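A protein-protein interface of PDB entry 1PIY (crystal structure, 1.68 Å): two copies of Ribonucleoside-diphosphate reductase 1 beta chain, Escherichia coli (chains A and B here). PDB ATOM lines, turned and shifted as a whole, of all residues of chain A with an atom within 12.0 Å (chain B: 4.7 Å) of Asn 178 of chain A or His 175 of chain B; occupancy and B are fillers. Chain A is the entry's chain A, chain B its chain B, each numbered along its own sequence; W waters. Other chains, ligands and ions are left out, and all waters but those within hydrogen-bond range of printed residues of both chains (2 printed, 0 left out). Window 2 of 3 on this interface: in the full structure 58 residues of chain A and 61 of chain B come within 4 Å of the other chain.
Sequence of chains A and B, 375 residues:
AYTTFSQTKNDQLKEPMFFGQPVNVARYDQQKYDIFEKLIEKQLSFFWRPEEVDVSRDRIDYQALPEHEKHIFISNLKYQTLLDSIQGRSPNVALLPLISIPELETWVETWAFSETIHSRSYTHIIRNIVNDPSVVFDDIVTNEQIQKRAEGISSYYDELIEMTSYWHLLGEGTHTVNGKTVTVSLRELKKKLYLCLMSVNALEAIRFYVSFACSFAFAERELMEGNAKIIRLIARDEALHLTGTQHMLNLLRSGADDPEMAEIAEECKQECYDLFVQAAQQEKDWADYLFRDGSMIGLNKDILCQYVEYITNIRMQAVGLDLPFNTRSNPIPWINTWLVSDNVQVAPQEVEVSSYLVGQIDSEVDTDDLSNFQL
ND2 of Asn 178 of chain A is in hydrogen-bond range of ND1 of His 175 of chain B, at 3.2 Å. The backbone NH of Asn 178 of chain A lies within hydrogen-bond range of the backbone carbonyl oxygen of Thr 176 of chain B (2.8 Å).
The backbone carbonyl oxygen (O) of Gly 171 of chain B lies within hydrogen-bond range of a ring nitrogen (NE2) of His 175 of chain B, at 2.9 Å. The backbone NH of Val 182 of chain B sits at hydrogen-bond distance from the backbone carbonyl oxygen of His 175 of chain B.
Among the printed residues, merely in contact across the chains: Thr 176 of chain A with Val 177 of chain B (3.3 Å), Val 177 of chain A with Thr 176 of chain B (3.5 Å), Leu 170 of chain A with Val 177 of chain B (3.5 Å), Val 177 of chain A with Leu 170 of chain B (3.6 Å) and Thr 176 of chain A with Thr 176 of chain B (3.6 Å).
Of the printed residues of chain B, Leu 170 of chain A touches Val 177. His 175 of chain A touches none of the printed residues of chain B. Of the printed residues of chain B, Thr 176 of chain A touches Thr 176 (3.6 Å) and Val 177 (3.3 Å). Of the printed residues of chain B, Val 177 of chain A touches Leu 170 and Thr 176. Of chain B, only His 175 (3.0 Å) and Thr 176 (2.8 Å) come within 4 Å of Asn 178 of chain A. Gly 179 of chain A touches none of the printed residues of chain B. Of chain A, only Val 177 comes within 4 Å of Leu 170 of chain B. No residue of chain A comes within 4 Å of Gly 171 of chain B. No residue of chain A comes within 4 Å of Gly 173 of chain B. No residue of chain A comes within 4 Å of Thr 174 of chain B. His 175 of chain B touches one residue of chain A. Thr 176 of chain B touches three residues of chain A. No residue of chain A comes within 4 Å of Thr 181 of chain B. The nearest residue of chain A that does not touch His 175 of chain B is Val 177 of chain A (6.1 Å). The nearest printed residue of chain B that does not touch Val 177 of chain A is Val 177 of chain B (4.6 Å).
Hydrophobic or aromatic side chains of chain B within 4 Å of the printed part of chain A: Leu 170, His 175 and Val 177. Hydrophobic or aromatic side chains of chain A that line the printed part of chain B: Leu 170 and Val 177. Among the printed residues, 7 pairs touch across the chains. Among the printed residues, no Asp or Glu carboxylate lies within 4 Å of a Lys or Arg side-chain nitrogen of the other chain.
Leu 170 of chain A touches Val 177 of chain B, and with the chains exchanged Val 177 of chain A touches Leu 170 of chain B. Thr 176 of chain B touches its own counterpart, Thr 176 of chain A. Thr 176 of chain A touches Val 177 of chain B, and with the chains exchanged Val 177 of chain A touches Thr 176 of chain B. 8 positions are printed for both chains.
Water W2 lies within hydrogen-bond range of OG1 of Thr 176 of chain B (2.8 Å), O of Thr 176 of chain A (2.8 Å), N of Asn 178 of chain A (3.1 Å) and N of Gly 179 of chain A (3.3 Å). Water W1 lies within hydrogen-bond range of ND1 of His 175 of chain B (2.9 Å), O of Thr 174 of chain B (3.2 Å) and OD1 of Asn 178 of chain A (3.4 Å).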
ATOM      1  N   GLU A 162     -17.102  -2.781  -4.234  1.00  0.00           N
ATOM      2  CA  GLU A 162     -16.529  -2.456  -2.934  1.00  0.00           C
ATOM      3  C   GLU A 162     -17.622  -2.370  -1.870  1.00  0.00           C
ATOM      4  O   GLU A 162     -17.466  -2.883  -0.761  1.00  0.00           O
ATOM      5  CB  GLU A 162     -15.764  -1.131  -2.999  1.00  0.00           C
ATOM      6  CG  GLU A 162     -15.056  -0.774  -1.692  1.00  0.00           C
ATOM      7  CD  GLU A 162     -14.352   0.575  -1.746  1.00  0.00           C
ATOM      8  OE1 GLU A 162     -13.504   0.783  -2.638  1.00  0.00           O
ATOM      9  OE2 GLU A 162     -14.647   1.432  -0.887  1.00  0.00           O
ATOM     10  N   TYR A 166     -18.267  -4.798   1.572  1.00  0.00           N
ATOM     11  CA  TYR A 166     -18.483  -4.290   2.924  1.00  0.00           C
ATOM     12  C   TYR A 166     -19.766  -4.877   3.504  1.00  0.00           C
ATOM     13  O   TYR A 166     -19.815  -5.261   4.676  1.00  0.00           O
ATOM     14  CB  TYR A 166     -18.550  -2.760   2.921  1.00  0.00           C
ATOM     15  CG  TYR A 166     -17.203  -2.106   3.133  1.00  0.00           C
ATOM     16  CD1 TYR A 166     -16.539  -2.232   4.348  1.00  0.00           C
ATOM     17  CD2 TYR A 166     -16.578  -1.388   2.110  1.00  0.00           C
ATOM     18  CE1 TYR A 166     -15.281  -1.661   4.548  1.00  0.00           C
ATOM     19  CE2 TYR A 166     -15.318  -0.815   2.298  1.00  0.00           C
ATOM     20  CZ  TYR A 166     -14.677  -0.959   3.522  1.00  0.00           C
ATOM     21  OH  TYR A 166     -13.423  -0.420   3.720  1.00  0.00           O
ATOM     22  N   LEU A 169     -19.327  -8.598   4.321  1.00  0.00           N
ATOM     23  CA  LEU A 169     -18.405  -8.776   5.437  1.00  0.00           C
ATOM     24  C   LEU A 169     -18.882  -8.264   6.789  1.00  0.00           C
ATOM     25  O   LEU A 169     -18.687  -8.924   7.811  1.00  0.00           O
ATOM     26  CB  LEU A 169     -17.059  -8.114   5.129  1.00  0.00           C
ATOM     27  CG  LEU A 169     -16.170  -8.777   4.077  1.00  0.00           C
ATOM     28  CD1 LEU A 169     -14.918  -7.936   3.857  1.00  0.00           C
ATOM     29  CD2 LEU A 169     -15.804 -10.177   4.537  1.00  0.00           C
ATOM     30  N   LEU A 170     -19.509  -7.094   6.789  1.00  0.00           N
ATOM     31  CA  LEU A 170     -19.946  -6.462   8.028  1.00  0.00           C
ATOM     32  C   LEU A 170     -21.445  -6.405   8.268  1.00  0.00           C
ATOM     33  O   LEU A 170     -21.894  -6.282   9.414  1.00  0.00           O
ATOM     34  CB  LEU A 170     -19.389  -5.041   8.077  1.00  0.00           C
ATOM     35  CG  LEU A 170     -17.898  -4.905   7.768  1.00  0.00           C
ATOM     36  CD1 LEU A 170     -17.515  -3.439   7.729  1.00  0.00           C
ATOM     37  CD2 LEU A 170     -17.088  -5.656   8.813  1.00  0.00           C
ATOM     38  N   THR A 174     -23.411   0.715  11.401  1.00  0.00           N
ATOM     39  CA  THR A 174     -22.351   1.716  11.420  1.00  0.00           C
ATOM     40  C   THR A 174     -21.196   1.010  12.114  1.00  0.00           C
ATOM     41  O   THR A 174     -21.316   0.589  13.270  1.00  0.00           O
ATOM     42  CB  THR A 174     -22.768   2.961  12.216  1.00  0.00           C
ATOM     43  OG1 THR A 174     -22.901   2.620  13.600  1.00  0.00           O
ATOM     44  CG2 THR A 174     -24.100   3.486  11.702  1.00  0.00           C
ATOM     45  N   HIS A 175     -20.085   0.880  11.402  1.00  0.00           N
ATOM     46  CA  HIS A 175     -18.929   0.160  11.915  1.00  0.00           C
ATOM     47  C   HIS A 175     -17.692   1.013  12.117  1.00  0.00           C
ATOM     48  O   HIS A 175     -17.643   2.168  11.706  1.00  0.00           O
ATOM     49  CB  HIS A 175     -18.593  -0.970  10.946  1.00  0.00           C
ATOM     50  CG  HIS A 175     -19.770  -1.818  10.583  1.00  0.00           C
ATOM     51  ND1 HIS A 175     -20.232  -2.835  11.388  1.00  0.00           N
ATOM     52  CD2 HIS A 175     -20.610  -1.766   9.522  1.00  0.00           C
ATOM     53  CE1 HIS A 175     -21.306  -3.375  10.840  1.00  0.00           C
ATOM     54  NE2 HIS A 175     -21.558  -2.744   9.706  1.00  0.00           N
ATOM     55  N   THR A 176     -16.690   0.410  12.747  1.00  0.00           N
ATOM     56  CA  THR A 176     -15.419   1.069  12.995  1.00  0.00           C
ATOM     57  C   THR A 176     -14.354   0.199  12.338  1.00  0.00           C
ATOM     58  O   THR A 176     -14.060  -0.896  12.812  1.00  0.00           O
ATOM     59  CB  THR A 176     -15.155   1.191  14.503  1.00  0.00           C
ATOM     60  OG1 THR A 176     -16.251   1.888  15.114  1.00  0.00           O
ATOM     61  CG2 THR A 176     -13.874   1.965  14.763  1.00  0.00           C
ATOM     62  N   VAL A 177     -13.800   0.686  11.231  1.00  0.00           N
ATOM     63  CA  VAL A 177     -12.783  -0.049  10.484  1.00  0.00           C
ATOM     64  C   VAL A 177     -11.483   0.739  10.513  1.00  0.00           C
ATOM     65  O   VAL A 177     -11.394   1.814   9.924  1.00  0.00           O
ATOM     66  CB  VAL A 177     -13.226  -0.245   9.019  1.00  0.00           C
ATOM     67  CG1 VAL A 177     -12.186  -1.043   8.258  1.00  0.00           C
ATOM     68  CG2 VAL A 177     -14.575  -0.949   8.983  1.00  0.00           C
ATOM     69  N   ASN A 178     -10.480   0.194  11.193  1.00  0.00           N
ATOM     70  CA  ASN A 178      -9.193   0.858  11.334  1.00  0.00           C
ATOM     71  C   ASN A 178      -9.344   2.281  11.859  1.00  0.00           C
ATOM     72  O   ASN A 178      -8.677   3.201  11.385  1.00  0.00           O
ATOM     73  CB  ASN A 178      -8.430   0.866  10.006  1.00  0.00           C
ATOM     74  CG  ASN A 178      -7.868  -0.493   9.660  1.00  0.00           C
ATOM     75  OD1 ASN A 178      -7.587  -1.296  10.551  1.00  0.00           O
ATOM     76  ND2 ASN A 178      -7.691  -0.759   8.368  1.00  0.00           N
ATOM     77  N   GLY A 179     -10.229   2.453  12.837  1.00  0.00           N
ATOM     78  CA  GLY A 179     -10.435   3.761  13.436  1.00  0.00           C
ATOM     79  C   GLY A 179     -11.326   4.724  12.676  1.00  0.00           C
ATOM     80  O   GLY A 179     -11.488   5.880  13.080  1.00  0.00           O
ATOM     81  N   LYS A 180     -11.901   4.269  11.572  1.00  0.00           N
ATOM     82  CA  LYS A 180     -12.777   5.128  10.797  1.00  0.00           C
ATOM     83  C   LYS A 180     -14.184   4.574  10.822  1.00  0.00           C
ATOM     84  O   LYS A 180     -14.391   3.362  10.874  1.00  0.00           O
ATOM     85  CB  LYS A 180     -12.278   5.258   9.358  1.00  0.00           C
ATOM     86  CG  LYS A 180     -10.926   5.956   9.266  1.00  0.00           C
ATOM     87  CD  LYS A 180     -10.623   6.462   7.860  1.00  0.00           C
ATOM     88  CE  LYS A 180     -10.482   5.328   6.853  1.00  0.00           C
ATOM     89  NZ  LYS A 180     -10.045   5.846   5.516  1.00  0.00           N
ATOM     90  N   THR A 181     -15.151   5.477  10.797  1.00  0.00           N
ATOM     91  CA  THR A 181     -16.545   5.093  10.830  1.00  0.00           C
ATOM     92  C   THR A 181     -17.006   4.785   9.414  1.00  0.00           C
ATOM     93  O   THR A 181     -16.897   5.624   8.518  1.00  0.00           O
ATOM     94  CB  THR A 181     -17.397   6.226  11.423  1.00  0.00           C
ATOM     95  OG1 THR A 181     -16.869   6.581  12.707  1.00  0.00           O
ATOM     96  CG2 THR A 181     -18.848   5.792  11.573  1.00  0.00           C
ATOM     97  N   VAL A 182     -17.508   3.571   9.228  1.00  0.00           N
ATOM     98  CA  VAL A 182     -17.998   3.119   7.934  1.00  0.00           C
ATOM     99  C   VAL A 182     -19.454   2.712   8.058  1.00  0.00           C
ATOM    100  O   VAL A 182     -19.810   1.866   8.882  1.00  0.00           O
ATOM    101  CB  VAL A 182     -17.181   1.918   7.425  1.00  0.00           C
ATOM    102  CG1 VAL A 182     -17.800   1.362   6.144  1.00  0.00           C
ATOM    103  CG2 VAL A 182     -15.738   2.351   7.179  1.00  0.00           C
ATOM    104  N   THR A 183     -20.298   3.332   7.244  1.00  0.00           N
ATOM    105  CA  THR A 183     -21.718   3.035   7.258  1.00  0.00           C
ATOM    106  C   THR A 183     -22.074   2.049   6.160  1.00  0.00           C
ATOM    107  O   THR A 183     -21.696   2.230   5.001  1.00  0.00           O
ATOM    108  CB  THR A 183     -22.562   4.306   7.049  1.00  0.00           C
ATOM    109  OG1 THR A 183     -22.258   5.256   8.077  1.00  0.00           O
ATOM    110  CG2 THR A 183     -24.039   3.972   7.102  1.00  0.00           C
ATOM    111  N   LEU B 170      -8.970  -3.969   2.631  1.00  0.00           N
ATOM    112  CA  LEU B 170      -7.996  -3.438   3.581  1.00  0.00           C
ATOM    113  C   LEU B 170      -6.518  -3.633   3.258  1.00  0.00           C
ATOM    114  O   LEU B 170      -5.665  -2.965   3.846  1.00  0.00           O
ATOM    115  CB  LEU B 170      -8.280  -4.025   4.966  1.00  0.00           C
ATOM    116  CG  LEU B 170      -9.718  -3.928   5.479  1.00  0.00           C
ATOM    117  CD1 LEU B 170      -9.842  -4.677   6.802  1.00  0.00           C
ATOM    118  CD2 LEU B 170     -10.107  -2.466   5.633  1.00  0.00           C
ATOM    119  N   GLY B 171      -6.207  -4.535   2.336  1.00  0.00           N
ATOM    120  CA  GLY B 171      -4.812  -4.773   2.014  1.00  0.00           C
ATOM    121  C   GLY B 171      -4.176  -5.599   3.121  1.00  0.00           C
ATOM    122  O   GLY B 171      -4.840  -5.967   4.093  1.00  0.00           O
ATOM    123  N   GLU B 172      -2.889  -5.893   2.979  1.00  0.00           N
ATOM    124  CA  GLU B 172      -2.181  -6.689   3.974  1.00  0.00           C
ATOM    125  C   GLU B 172      -1.927  -5.913   5.246  1.00  0.00           C
ATOM    126  O   GLU B 172      -1.656  -4.714   5.200  1.00  0.00           O
ATOM    127  CB  GLU B 172      -0.825  -7.147   3.447  1.00  0.00           C
ATOM    128  CG  GLU B 172      -0.861  -8.120   2.297  1.00  0.00           C
ATOM    129  CD  GLU B 172       0.485  -8.781   2.103  1.00  0.00           C
ATOM    130  OE1 GLU B 172       0.867  -9.589   2.978  1.00  0.00           O
ATOM    131  OE2 GLU B 172       1.166  -8.483   1.093  1.00  0.00           O
ATOM    132  N   GLY B 173      -1.979  -6.612   6.375  1.00  0.00           N
ATOM    133  CA  GLY B 173      -1.720  -5.962   7.641  1.00  0.00           C
ATOM    134  C   GLY B 173      -2.578  -6.437   8.787  1.00  0.00           C
ATOM    135  O   GLY B 173      -3.351  -7.391   8.664  1.00  0.00           O
ATOM    136  N   THR B 174      -2.411  -5.761   9.919  1.00  0.00           N
ATOM    137  CA  THR B 174      -3.161  -6.048  11.132  1.00  0.00           C
ATOM    138  C   THR B 174      -4.129  -4.885  11.279  1.00  0.00           C
ATOM    139  O   THR B 174      -3.725  -3.755  11.577  1.00  0.00           O
ATOM    140  CB  THR B 174      -2.236  -6.097  12.357  1.00  0.00           C
ATOM    141  OG1 THR B 174      -1.148  -6.994  12.095  1.00  0.00           O
ATOM    142  CG2 THR B 174      -3.000  -6.583  13.578  1.00  0.00           C
ATOM    143  N   HIS B 175      -5.405  -5.171  11.059  1.00  0.00           N
ATOM    144  CA  HIS B 175      -6.453  -4.163  11.117  1.00  0.00           C
ATOM    145  C   HIS B 175      -7.381  -4.409  12.294  1.00  0.00           C
ATOM    146  O   HIS B 175      -7.273  -5.419  12.980  1.00  0.00           O
ATOM    147  CB  HIS B 175      -7.278  -4.225   9.830  1.00  0.00           C
ATOM    148  CG  HIS B 175      -6.449  -4.340   8.589  1.00  0.00           C
ATOM    149  ND1 HIS B 175      -5.685  -3.302   8.104  1.00  0.00           N
ATOM    150  CD2 HIS B 175      -6.249  -5.382   7.746  1.00  0.00           C
ATOM    151  CE1 HIS B 175      -5.051  -3.698   7.015  1.00  0.00           C
ATOM    152  NE2 HIS B 175      -5.375  -4.956   6.776  1.00  0.00           N
ATOM    153  N   THR B 176      -8.295  -3.474  12.522  1.00  0.00           N
ATOM    154  CA  THR B 176      -9.278  -3.629  13.583  1.00  0.00           C
ATOM    155  C   THR B 176     -10.649  -3.360  12.988  1.00  0.00           C
ATOM    156  O   THR B 176     -10.824  -2.445  12.179  1.00  0.00           O
ATOM    157  CB  THR B 176      -9.055  -2.644  14.756  1.00  0.00           C
ATOM    158  OG1 THR B 176      -9.080  -1.302  14.267  1.00  0.00           O
ATOM    159  CG2 THR B 176      -7.733  -2.916  15.437  1.00  0.00           C
ATOM    160  N   VAL B 177     -11.612  -4.182  13.372  1.00  0.00           N
ATOM    161  CA  VAL B 177     -12.976  -4.036  12.898  1.00  0.00           C
ATOM    162  C   VAL B 177     -13.886  -4.237  14.098  1.00  0.00           C
ATOM    163  O   VAL B 177     -13.941  -5.324  14.669  1.00  0.00           O
ATOM    164  CB  VAL B 177     -13.321  -5.092  11.815  1.00  0.00           C
ATOM    165  CG1 VAL B 177     -14.771  -4.932  11.382  1.00  0.00           C
ATOM    166  CG2 VAL B 177     -12.385  -4.943  10.619  1.00  0.00           C
ATOM    167  N   LYS B 180     -12.328  -5.822  17.136  1.00  0.00           N
ATOM    168  CA  LYS B 180     -11.596  -7.064  16.919  1.00  0.00           C
ATOM    169  C   LYS B 180     -10.436  -6.897  15.957  1.00  0.00           C
ATOM    170  O   LYS B 180     -10.519  -6.129  15.000  1.00  0.00           O
ATOM    171  CB  LYS B 180     -12.528  -8.143  16.378  1.00  0.00           C
ATOM    172  CG  LYS B 180     -13.569  -8.595  17.370  1.00  0.00           C
ATOM    173  CD  LYS B 180     -14.498  -9.624  16.760  1.00  0.00           C
ATOM    174  CE  LYS B 180     -15.457 -10.148  17.806  1.00  0.00           C
ATOM    175  NZ  LYS B 180     -14.701 -10.743  18.943  1.00  0.00           N
ATOM    176  N   THR B 181      -9.351  -7.619  16.211  1.00  0.00           N
ATOM    177  CA  THR B 181      -8.200  -7.549  15.328  1.00  0.00           C
ATOM    178  C   THR B 181      -8.474  -8.448  14.129  1.00  0.00           C
ATOM    179  O   THR B 181      -8.949  -9.575  14.282  1.00  0.00           O
ATOM    180  CB  THR B 181      -6.909  -8.042  16.014  1.00  0.00           C
ATOM    181  OG1 THR B 181      -6.685  -7.294  17.216  1.00  0.00           O
ATOM    182  CG2 THR B 181      -5.722  -7.857  15.087  1.00  0.00           C
ATOM    183  N   VAL B 182      -8.195  -7.940  12.934  1.00  0.00           N
ATOM    184  CA  VAL B 182      -8.386  -8.716  11.715  1.00  0.00           C
ATOM    185  C   VAL B 182      -7.081  -8.673  10.938  1.00  0.00           C
ATOM    186  O   VAL B 182      -6.680  -7.623  10.422  1.00  0.00           O
ATOM    187  CB  VAL B 182      -9.522  -8.147  10.839  1.00  0.00           C
ATOM    188  CG1 VAL B 182      -9.599  -8.913   9.527  1.00  0.00           C
ATOM    189  CG2 VAL B 182     -10.846  -8.246  11.582  1.00  0.00           C
ATOM    190  N   VAL B 184      -4.735  -9.648   7.800  1.00  0.00           N
ATOM    191  CA  VAL B 184      -4.806  -9.983   6.384  1.00  0.00           C
ATOM    192  C   VAL B 184      -3.399 -10.286   5.890  1.00  0.00           C
ATOM    193  O   VAL B 184      -2.519  -9.427   5.927  1.00  0.00           O
ATOM    194  CB  VAL B 184      -5.403  -8.821   5.555  1.00  0.00           C
ATOM    195  CG1 VAL B 184      -5.335  -9.146   4.065  1.00  0.00           C
ATOM    196  CG2 VAL B 184      -6.853  -8.580   5.969  1.00  0.00           C
HETATM  197  O   HOH W   1      -4.326  -1.253   9.605  1.00  0.00           O
HETATM  198  O   HOH W   2     -11.611  -0.211  14.092  1.00  0.00           O
